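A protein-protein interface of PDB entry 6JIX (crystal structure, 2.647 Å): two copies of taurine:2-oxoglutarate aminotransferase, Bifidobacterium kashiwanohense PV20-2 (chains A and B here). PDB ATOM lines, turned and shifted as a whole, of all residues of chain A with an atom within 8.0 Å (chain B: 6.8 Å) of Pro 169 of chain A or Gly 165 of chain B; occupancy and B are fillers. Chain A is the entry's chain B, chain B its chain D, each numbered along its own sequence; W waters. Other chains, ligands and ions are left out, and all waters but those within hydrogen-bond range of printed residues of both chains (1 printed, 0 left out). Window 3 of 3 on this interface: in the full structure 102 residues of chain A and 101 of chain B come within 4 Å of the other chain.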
ATOM      1  N   ILE A 124      -0.359   9.869 -14.136  1.00  0.00           N
ATOM      2  CA  ILE A 124      -0.242  11.250 -13.680  1.00  0.00           C
ATOM      3  C   ILE A 124      -0.259  12.215 -14.864  1.00  0.00           C
ATOM      4  O   ILE A 124      -1.016  13.194 -14.874  1.00  0.00           O
ATOM      5  CB  ILE A 124       1.037  11.421 -12.850  1.00  0.00           C
ATOM      6  CG1 ILE A 124       0.914  10.689 -11.525  1.00  0.00           C
ATOM      7  CG2 ILE A 124       1.365  12.906 -12.670  1.00  0.00           C
ATOM      8  CD1 ILE A 124       2.251  10.485 -10.866  1.00  0.00           C
ATOM      9  N   ARG A 128      -3.173  15.171 -15.614  1.00  0.00           N
ATOM     10  CA  ARG A 128      -2.898  16.599 -15.741  1.00  0.00           C
ATOM     11  C   ARG A 128      -3.337  17.122 -17.111  1.00  0.00           C
ATOM     12  O   ARG A 128      -3.903  18.219 -17.212  1.00  0.00           O
ATOM     13  CB  ARG A 128      -1.410  16.869 -15.493  1.00  0.00           C
ATOM     14  CG  ARG A 128      -1.048  17.113 -14.041  1.00  0.00           C
ATOM     15  CD  ARG A 128       0.389  16.712 -13.749  1.00  0.00           C
ATOM     16  NE  ARG A 128       0.784  17.038 -12.380  1.00  0.00           N
ATOM     17  CZ  ARG A 128       2.005  16.855 -11.878  1.00  0.00           C
ATOM     18  NH1 ARG A 128       2.970  16.340 -12.635  1.00  0.00           N
ATOM     19  NH2 ARG A 128       2.266  17.207 -10.621  1.00  0.00           N
ATOM     20  N   GLY A 132      -6.458  19.400 -17.096  1.00  0.00           N
ATOM     21  CA  GLY A 132      -5.845  20.709 -17.103  1.00  0.00           C
ATOM     22  C   GLY A 132      -5.428  21.238 -15.747  1.00  0.00           C
ATOM     23  O   GLY A 132      -5.087  22.418 -15.638  1.00  0.00           O
ATOM     24  N   ARG A 133      -5.468  20.421 -14.707  1.00  0.00           N
ATOM     25  CA  ARG A 133      -5.157  20.875 -13.361  1.00  0.00           C
ATOM     26  C   ARG A 133      -3.782  20.364 -12.947  1.00  0.00           C
ATOM     27  O   ARG A 133      -3.363  19.297 -13.398  1.00  0.00           O
ATOM     28  CB  ARG A 133      -6.207  20.380 -12.358  1.00  0.00           C
ATOM     29  CG  ARG A 133      -7.656  20.560 -12.797  1.00  0.00           C
ATOM     30  CD  ARG A 133      -8.577  19.783 -11.887  1.00  0.00           C
ATOM     31  NE  ARG A 133      -9.968  20.095 -12.149  1.00  0.00           N
ATOM     32  CZ  ARG A 133     -10.971  19.700 -11.377  1.00  0.00           C
ATOM     33  NH1 ARG A 133     -10.732  18.980 -10.291  1.00  0.00           N
ATOM     34  NH2 ARG A 133     -12.213  20.022 -11.697  1.00  0.00           N
ATOM     35  N   PRO A 134      -3.063  21.066 -12.067  1.00  0.00           N
ATOM     36  CA  PRO A 134      -1.659  20.683 -11.822  1.00  0.00           C
ATOM     37  C   PRO A 134      -1.425  19.624 -10.746  1.00  0.00           C
ATOM     38  O   PRO A 134      -0.443  18.883 -10.832  1.00  0.00           O
ATOM     39  CB  PRO A 134      -1.015  22.017 -11.418  1.00  0.00           C
ATOM     40  CG  PRO A 134      -2.140  22.783 -10.744  1.00  0.00           C
ATOM     41  CD  PRO A 134      -3.435  22.319 -11.375  1.00  0.00           C
ATOM     42  N   LYS A 135      -2.295  19.531  -9.740  1.00  0.00           N
ATOM     43  CA  LYS A 135      -1.967  18.842  -8.495  1.00  0.00           C
ATOM     44  C   LYS A 135      -2.391  17.379  -8.499  1.00  0.00           C
ATOM     45  O   LYS A 135      -3.449  17.025  -9.025  1.00  0.00           O
ATOM     46  CB  LYS A 135      -2.630  19.553  -7.313  1.00  0.00           C
ATOM     47  CG  LYS A 135      -1.922  20.821  -6.878  1.00  0.00           C
ATOM     48  CD  LYS A 135      -2.724  21.571  -5.828  1.00  0.00           C
ATOM     49  CE  LYS A 135      -2.450  23.077  -5.896  1.00  0.00           C
ATOM     50  NZ  LYS A 135      -2.661  23.746  -4.585  1.00  0.00           N
ATOM     51  N   ILE A 136      -1.579  16.549  -7.844  1.00  0.00           N
ATOM     52  CA  ILE A 136      -1.856  15.135  -7.604  1.00  0.00           C
ATOM     53  C   ILE A 136      -1.894  14.924  -6.095  1.00  0.00           C
ATOM     54  O   ILE A 136      -0.930  15.266  -5.398  1.00  0.00           O
ATOM     55  CB  ILE A 136      -0.787  14.216  -8.224  1.00  0.00           C
ATOM     56  CG1 ILE A 136      -0.673  14.412  -9.741  1.00  0.00           C
ATOM     57  CG2 ILE A 136      -1.043  12.763  -7.809  1.00  0.00           C
ATOM     58  CD1 ILE A 136      -1.885  13.956 -10.542  1.00  0.00           C
ATOM     59  N   ASN A 152       7.914  10.912  -6.121  1.00  0.00           N
ATOM     60  CA  ASN A 152       7.291  12.072  -5.497  1.00  0.00           C
ATOM     61  C   ASN A 152       5.849  11.761  -5.110  1.00  0.00           C
ATOM     62  O   ASN A 152       5.361  12.226  -4.071  1.00  0.00           O
ATOM     63  CB  ASN A 152       7.358  13.287  -6.424  1.00  0.00           C
ATOM     64  CG  ASN A 152       8.599  14.120  -6.199  1.00  0.00           C
ATOM     65  OD1 ASN A 152       8.658  14.969  -5.296  1.00  0.00           O
ATOM     66  ND2 ASN A 152       9.604  13.882  -7.016  1.00  0.00           N
ATOM     67  N   GLY A 166      15.024  18.873  -4.419  1.00  0.00           N
ATOM     68  CA  GLY A 166      13.683  19.451  -4.327  1.00  0.00           C
ATOM     69  C   GLY A 166      12.514  18.520  -4.644  1.00  0.00           C
ATOM     70  O   GLY A 166      12.664  17.557  -5.407  1.00  0.00           O
ATOM     71  N   SER A 167      11.345  18.776  -4.047  1.00  0.00           N
ATOM     72  CA  SER A 167      10.144  18.023  -4.385  1.00  0.00           C
ATOM     73  C   SER A 167       9.593  18.521  -5.709  1.00  0.00           C
ATOM     74  O   SER A 167       9.566  19.727  -5.963  1.00  0.00           O
ATOM     75  CB  SER A 167       9.065  18.200  -3.320  1.00  0.00           C
ATOM     76  OG  SER A 167       9.634  18.295  -2.030  1.00  0.00           O
ATOM     77  N   ALA A 168       9.118  17.604  -6.540  1.00  0.00           N
ATOM     78  CA  ALA A 168       8.504  18.045  -7.781  1.00  0.00           C
ATOM     79  C   ALA A 168       7.163  18.706  -7.456  1.00  0.00           C
ATOM     80  O   ALA A 168       6.420  18.213  -6.599  1.00  0.00           O
ATOM     81  CB  ALA A 168       8.328  16.872  -8.745  1.00  0.00           C
ATOM     82  N   PRO A 169       6.818  19.810  -8.120  1.00  0.00           N
ATOM     83  CA  PRO A 169       5.617  20.554  -7.722  1.00  0.00           C
ATOM     84  C   PRO A 169       4.334  19.793  -8.029  1.00  0.00           C
ATOM     85  O   PRO A 169       4.258  18.977  -8.954  1.00  0.00           O
ATOM     86  CB  PRO A 169       5.704  21.850  -8.544  1.00  0.00           C
ATOM     87  CG  PRO A 169       7.074  21.860  -9.149  1.00  0.00           C
ATOM     88  CD  PRO A 169       7.482  20.424  -9.276  1.00  0.00           C
ATOM     89  N   GLY A 170       3.307  20.091  -7.247  1.00  0.00           N
ATOM     90  CA  GLY A 170       1.995  19.553  -7.516  1.00  0.00           C
ATOM     91  C   GLY A 170       1.728  18.205  -6.907  1.00  0.00           C
ATOM     92  O   GLY A 170       0.779  17.533  -7.326  1.00  0.00           O
ATOM     93  N   PHE A 171       2.532  17.782  -5.940  1.00  0.00           N
ATOM     94  CA  PHE A 171       2.358  16.493  -5.283  1.00  0.00           C
ATOM     95  C   PHE A 171       2.019  16.737  -3.814  1.00  0.00           C
ATOM     96  O   PHE A 171       2.914  16.994  -3.002  1.00  0.00           O
ATOM     97  CB  PHE A 171       3.607  15.638  -5.435  1.00  0.00           C
ATOM     98  CG  PHE A 171       3.778  15.080  -6.805  1.00  0.00           C
ATOM     99  CD1 PHE A 171       3.116  13.913  -7.176  1.00  0.00           C
ATOM    100  CD2 PHE A 171       4.594  15.731  -7.740  1.00  0.00           C
ATOM    101  CE1 PHE A 171       3.269  13.400  -8.455  1.00  0.00           C
ATOM    102  CE2 PHE A 171       4.751  15.228  -9.027  1.00  0.00           C
ATOM    103  CZ  PHE A 171       4.097  14.064  -9.390  1.00  0.00           C
ATOM    104  N   VAL A 172       0.730  16.623  -3.484  1.00  0.00           N
ATOM    105  CA  VAL A 172       0.218  16.818  -2.134  1.00  0.00           C
ATOM    106  C   VAL A 172      -0.100  15.462  -1.518  1.00  0.00           C
ATOM    107  O   VAL A 172      -0.805  14.641  -2.123  1.00  0.00           O
ATOM    108  CB  VAL A 172      -1.037  17.707  -2.138  1.00  0.00           C
ATOM    109  CG1 VAL A 172      -1.404  18.100  -0.709  1.00  0.00           C
ATOM    110  CG2 VAL A 172      -0.816  18.927  -2.977  1.00  0.00           C
ATOM    111  N   SER A 212      -7.901  22.676  -8.652  1.00  0.00           N
ATOM    112  CA  SER A 212      -6.515  22.507  -9.066  1.00  0.00           C
ATOM    113  C   SER A 212      -6.001  21.081  -8.896  1.00  0.00           C
ATOM    114  O   SER A 212      -4.814  20.834  -9.154  1.00  0.00           O
ATOM    115  CB  SER A 212      -5.612  23.464  -8.285  1.00  0.00           C
ATOM    116  OG  SER A 212      -5.415  22.989  -6.964  1.00  0.00           O
ATOM    117  N   ALA B 161       4.543  18.967 -22.053  1.00  0.00           N
ATOM    118  CA  ALA B 161       3.426  18.296 -21.385  1.00  0.00           C
ATOM    119  C   ALA B 161       3.795  17.852 -19.969  1.00  0.00           C
ATOM    120  O   ALA B 161       2.996  18.000 -19.033  1.00  0.00           O
ATOM    121  CB  ALA B 161       2.962  17.098 -22.222  1.00  0.00           C
ATOM    122  N   THR B 162       4.989  17.270 -19.798  1.00  0.00           N
ATOM    123  CA  THR B 162       5.421  16.834 -18.472  1.00  0.00           C
ATOM    124  C   THR B 162       5.522  18.005 -17.498  1.00  0.00           C
ATOM    125  O   THR B 162       5.303  17.836 -16.289  1.00  0.00           O
ATOM    126  CB  THR B 162       6.763  16.104 -18.575  1.00  0.00           C
ATOM    127  OG1 THR B 162       6.619  14.930 -19.392  1.00  0.00           O
ATOM    128  CG2 THR B 162       7.278  15.708 -17.189  1.00  0.00           C
ATOM    129  N   GLU B 163       5.836  19.196 -18.008  1.00  0.00           N
ATOM    130  CA  GLU B 163       5.993  20.392 -17.192  1.00  0.00           C
ATOM    131  C   GLU B 163       4.662  20.977 -16.726  1.00  0.00           C
ATOM    132  O   GLU B 163       4.665  21.939 -15.952  1.00  0.00           O
ATOM    133  CB  GLU B 163       6.792  21.431 -17.970  1.00  0.00           C
ATOM    134  CG  GLU B 163       8.288  21.188 -17.913  1.00  0.00           C
ATOM    135  CD  GLU B 163       9.093  22.248 -18.658  1.00  0.00           C
ATOM    136  OE1 GLU B 163       8.497  22.975 -19.501  1.00  0.00           O
ATOM    137  OE2 GLU B 163      10.323  22.335 -18.394  1.00  0.00           O
ATOM    138  N   LEU B 164       3.536  20.412 -17.167  1.00  0.00           N
ATOM    139  CA  LEU B 164       2.237  20.752 -16.601  1.00  0.00           C
ATOM    140  C   LEU B 164       2.240  20.514 -15.099  1.00  0.00           C
ATOM    141  O   LEU B 164       2.623  19.436 -14.633  1.00  0.00           O
ATOM    142  CB  LEU B 164       1.154  19.898 -17.243  1.00  0.00           C
ATOM    143  CG  LEU B 164       0.823  20.277 -18.671  1.00  0.00           C
ATOM    144  CD1 LEU B 164       0.020  19.161 -19.356  1.00  0.00           C
ATOM    145  CD2 LEU B 164       0.075  21.618 -18.639  1.00  0.00           C
ATOM    146  N   GLY B 165       1.797  21.512 -14.336  1.00  0.00           N
ATOM    147  CA  GLY B 165       1.929  21.448 -12.894  1.00  0.00           C
ATOM    148  C   GLY B 165       3.214  22.028 -12.347  1.00  0.00           C
ATOM    149  O   GLY B 165       3.334  22.164 -11.122  1.00  0.00           O
ATOM    150  N   GLY B 166       4.175  22.354 -13.215  1.00  0.00           N
ATOM    151  CA  GLY B 166       5.450  22.940 -12.847  1.00  0.00           C
ATOM    152  C   GLY B 166       6.637  22.100 -13.278  1.00  0.00           C
ATOM    153  O   GLY B 166       6.548  20.872 -13.327  1.00  0.00           O
ATOM    154  N   SER B 167       7.762  22.753 -13.577  1.00  0.00           N
ATOM    155  CA  SER B 167       9.007  22.062 -13.881  1.00  0.00           C
ATOM    156  C   SER B 167       9.634  21.535 -12.593  1.00  0.00           C
ATOM    157  O   SER B 167       9.505  22.139 -11.524  1.00  0.00           O
ATOM    158  CB  SER B 167       9.986  22.987 -14.617  1.00  0.00           C
ATOM    159  OG  SER B 167      10.663  23.881 -13.734  1.00  0.00           O
ATOM    160  N   ALA B 168      10.283  20.377 -12.698  1.00  0.00           N
ATOM    161  CA  ALA B 168      10.943  19.789 -11.542  1.00  0.00           C
ATOM    162  C   ALA B 168      12.168  20.616 -11.154  1.00  0.00           C
ATOM    163  O   ALA B 168      12.877  21.133 -12.029  1.00  0.00           O
ATOM    164  CB  ALA B 168      11.361  18.345 -11.838  1.00  0.00           C
ATOM    165  N   PRO B 169      12.432  20.785  -9.858  1.00  0.00           N
ATOM    166  CA  PRO B 169      13.563  21.628  -9.456  1.00  0.00           C
ATOM    167  C   PRO B 169      14.886  20.958  -9.802  1.00  0.00           C
ATOM    168  O   PRO B 169      15.003  19.731  -9.831  1.00  0.00           O
ATOM    169  CB  PRO B 169      13.384  21.769  -7.938  1.00  0.00           C
ATOM    170  CG  PRO B 169      12.632  20.539  -7.530  1.00  0.00           C
ATOM    171  CD  PRO B 169      11.721  20.210  -8.701  1.00  0.00           C
HETATM  172  O   HOH W   1       4.354  19.266 -12.816  1.00  0.00           O
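Among the printed residues, merely in contact across the chains: Arg 128 of chain A with Leu 164 of chain B (3.6 Å), Pro 134 of chain A with Gly 165 of chain B (3.3 Å), Gly 166 of chain A with Pro 169 of chain B (3.5 Å), Ser 167 of chain A with Pro 169 of chain B (3.5 Å), Ala 168 of chain A with Pro 169 of chain B (3.99 Å), Pro 169 of chain A with Gly 165 of chain B (3.5 Å) and Pro 169 of chain A with Ser 167 of chain B (3.4 Å).
O of Pro 134 of chain A is in hydrogen-bond range of NE of Arg 128 of chain A, at 2.7 Å.
NH2 of Arg 128 of chain A is in hydrogen-bond range of O of Pro 169 of chain A (3.1 Å).
The side-chain amide oxygen (OD1) of Asn 152 of chain A lies within hydrogen-bond range of the backbone NH (N) of Ala 168 of chain A (2.9 Å).
Of the 16 printed residues of chain A, 6 touch a printed residue of chain B.
Along chain B the printed residues that touch a printed residue of chain A span positions 164 to 169.
Among the printed residues, no Asp or Glu carboxylate lies within 4 Å of a Lys or Arg side-chain nitrogen of the other chain.
Of chain B, only Gly 165 (3.5 Å) and Ser 167 (3.4 Å) come within 4 Å of Pro 169 of chain A.
Printed residues of chain A within 4 Å of Gly 165 of chain B: Pro 134 (3.3 Å) and Pro 169 (3.5 Å).
No residue of chain A comes within 4 Å of Gly 166 of chain B.
Printed residues of chain B within 4 Å of Gly 166 of chain A: Pro 169.
Of the printed residues of chain A, Ser 167 of chain B touches Pro 169 (3.4 Å).
Printed residues of chain B within 4 Å of Arg 128 of chain A: Leu 164 (3.6 Å).
Thr 162 of chain B touches none of the printed residues of chain A.
The nearest printed residue of chain B that does not touch Pro 169 of chain A is Gly 166 of chain B (4.2 Å).
The nearest printed residue of chain A that does not touch Leu 164 of chain B is Pro 134 of chain A (4.9 Å).
Gly 166 of chain A touches Pro 169 of chain B, but with the chains exchanged Pro 169 of chain A does not touch Gly 166 of chain B (4.2 Å).
Ser 167 of chain A touches Pro 169 of chain B, and with the chains exchanged Pro 169 of chain A touches Ser 167 of chain B.
Ala 168 of chain A touches Pro 169 of chain B, but with the chains exchanged Pro 169 of chain A does not touch Ala 168 of chain B (4.2 Å).
Positions printed for both chains: 166, 167, 168 and 169.
Of the 7 pairs that touch across the chains among the printed residues, 2 have their exchanged pair printed and touching as well.
Water W1 lies within hydrogen-bond range of the backbone carbonyl oxygen of Leu 164 of chain B (2.5 Å), the backbone carbonyl oxygen of Gly 166 of chain B (2.8 Å) and the guanidinium group of Arg 128 of chain A (3.2 Å).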
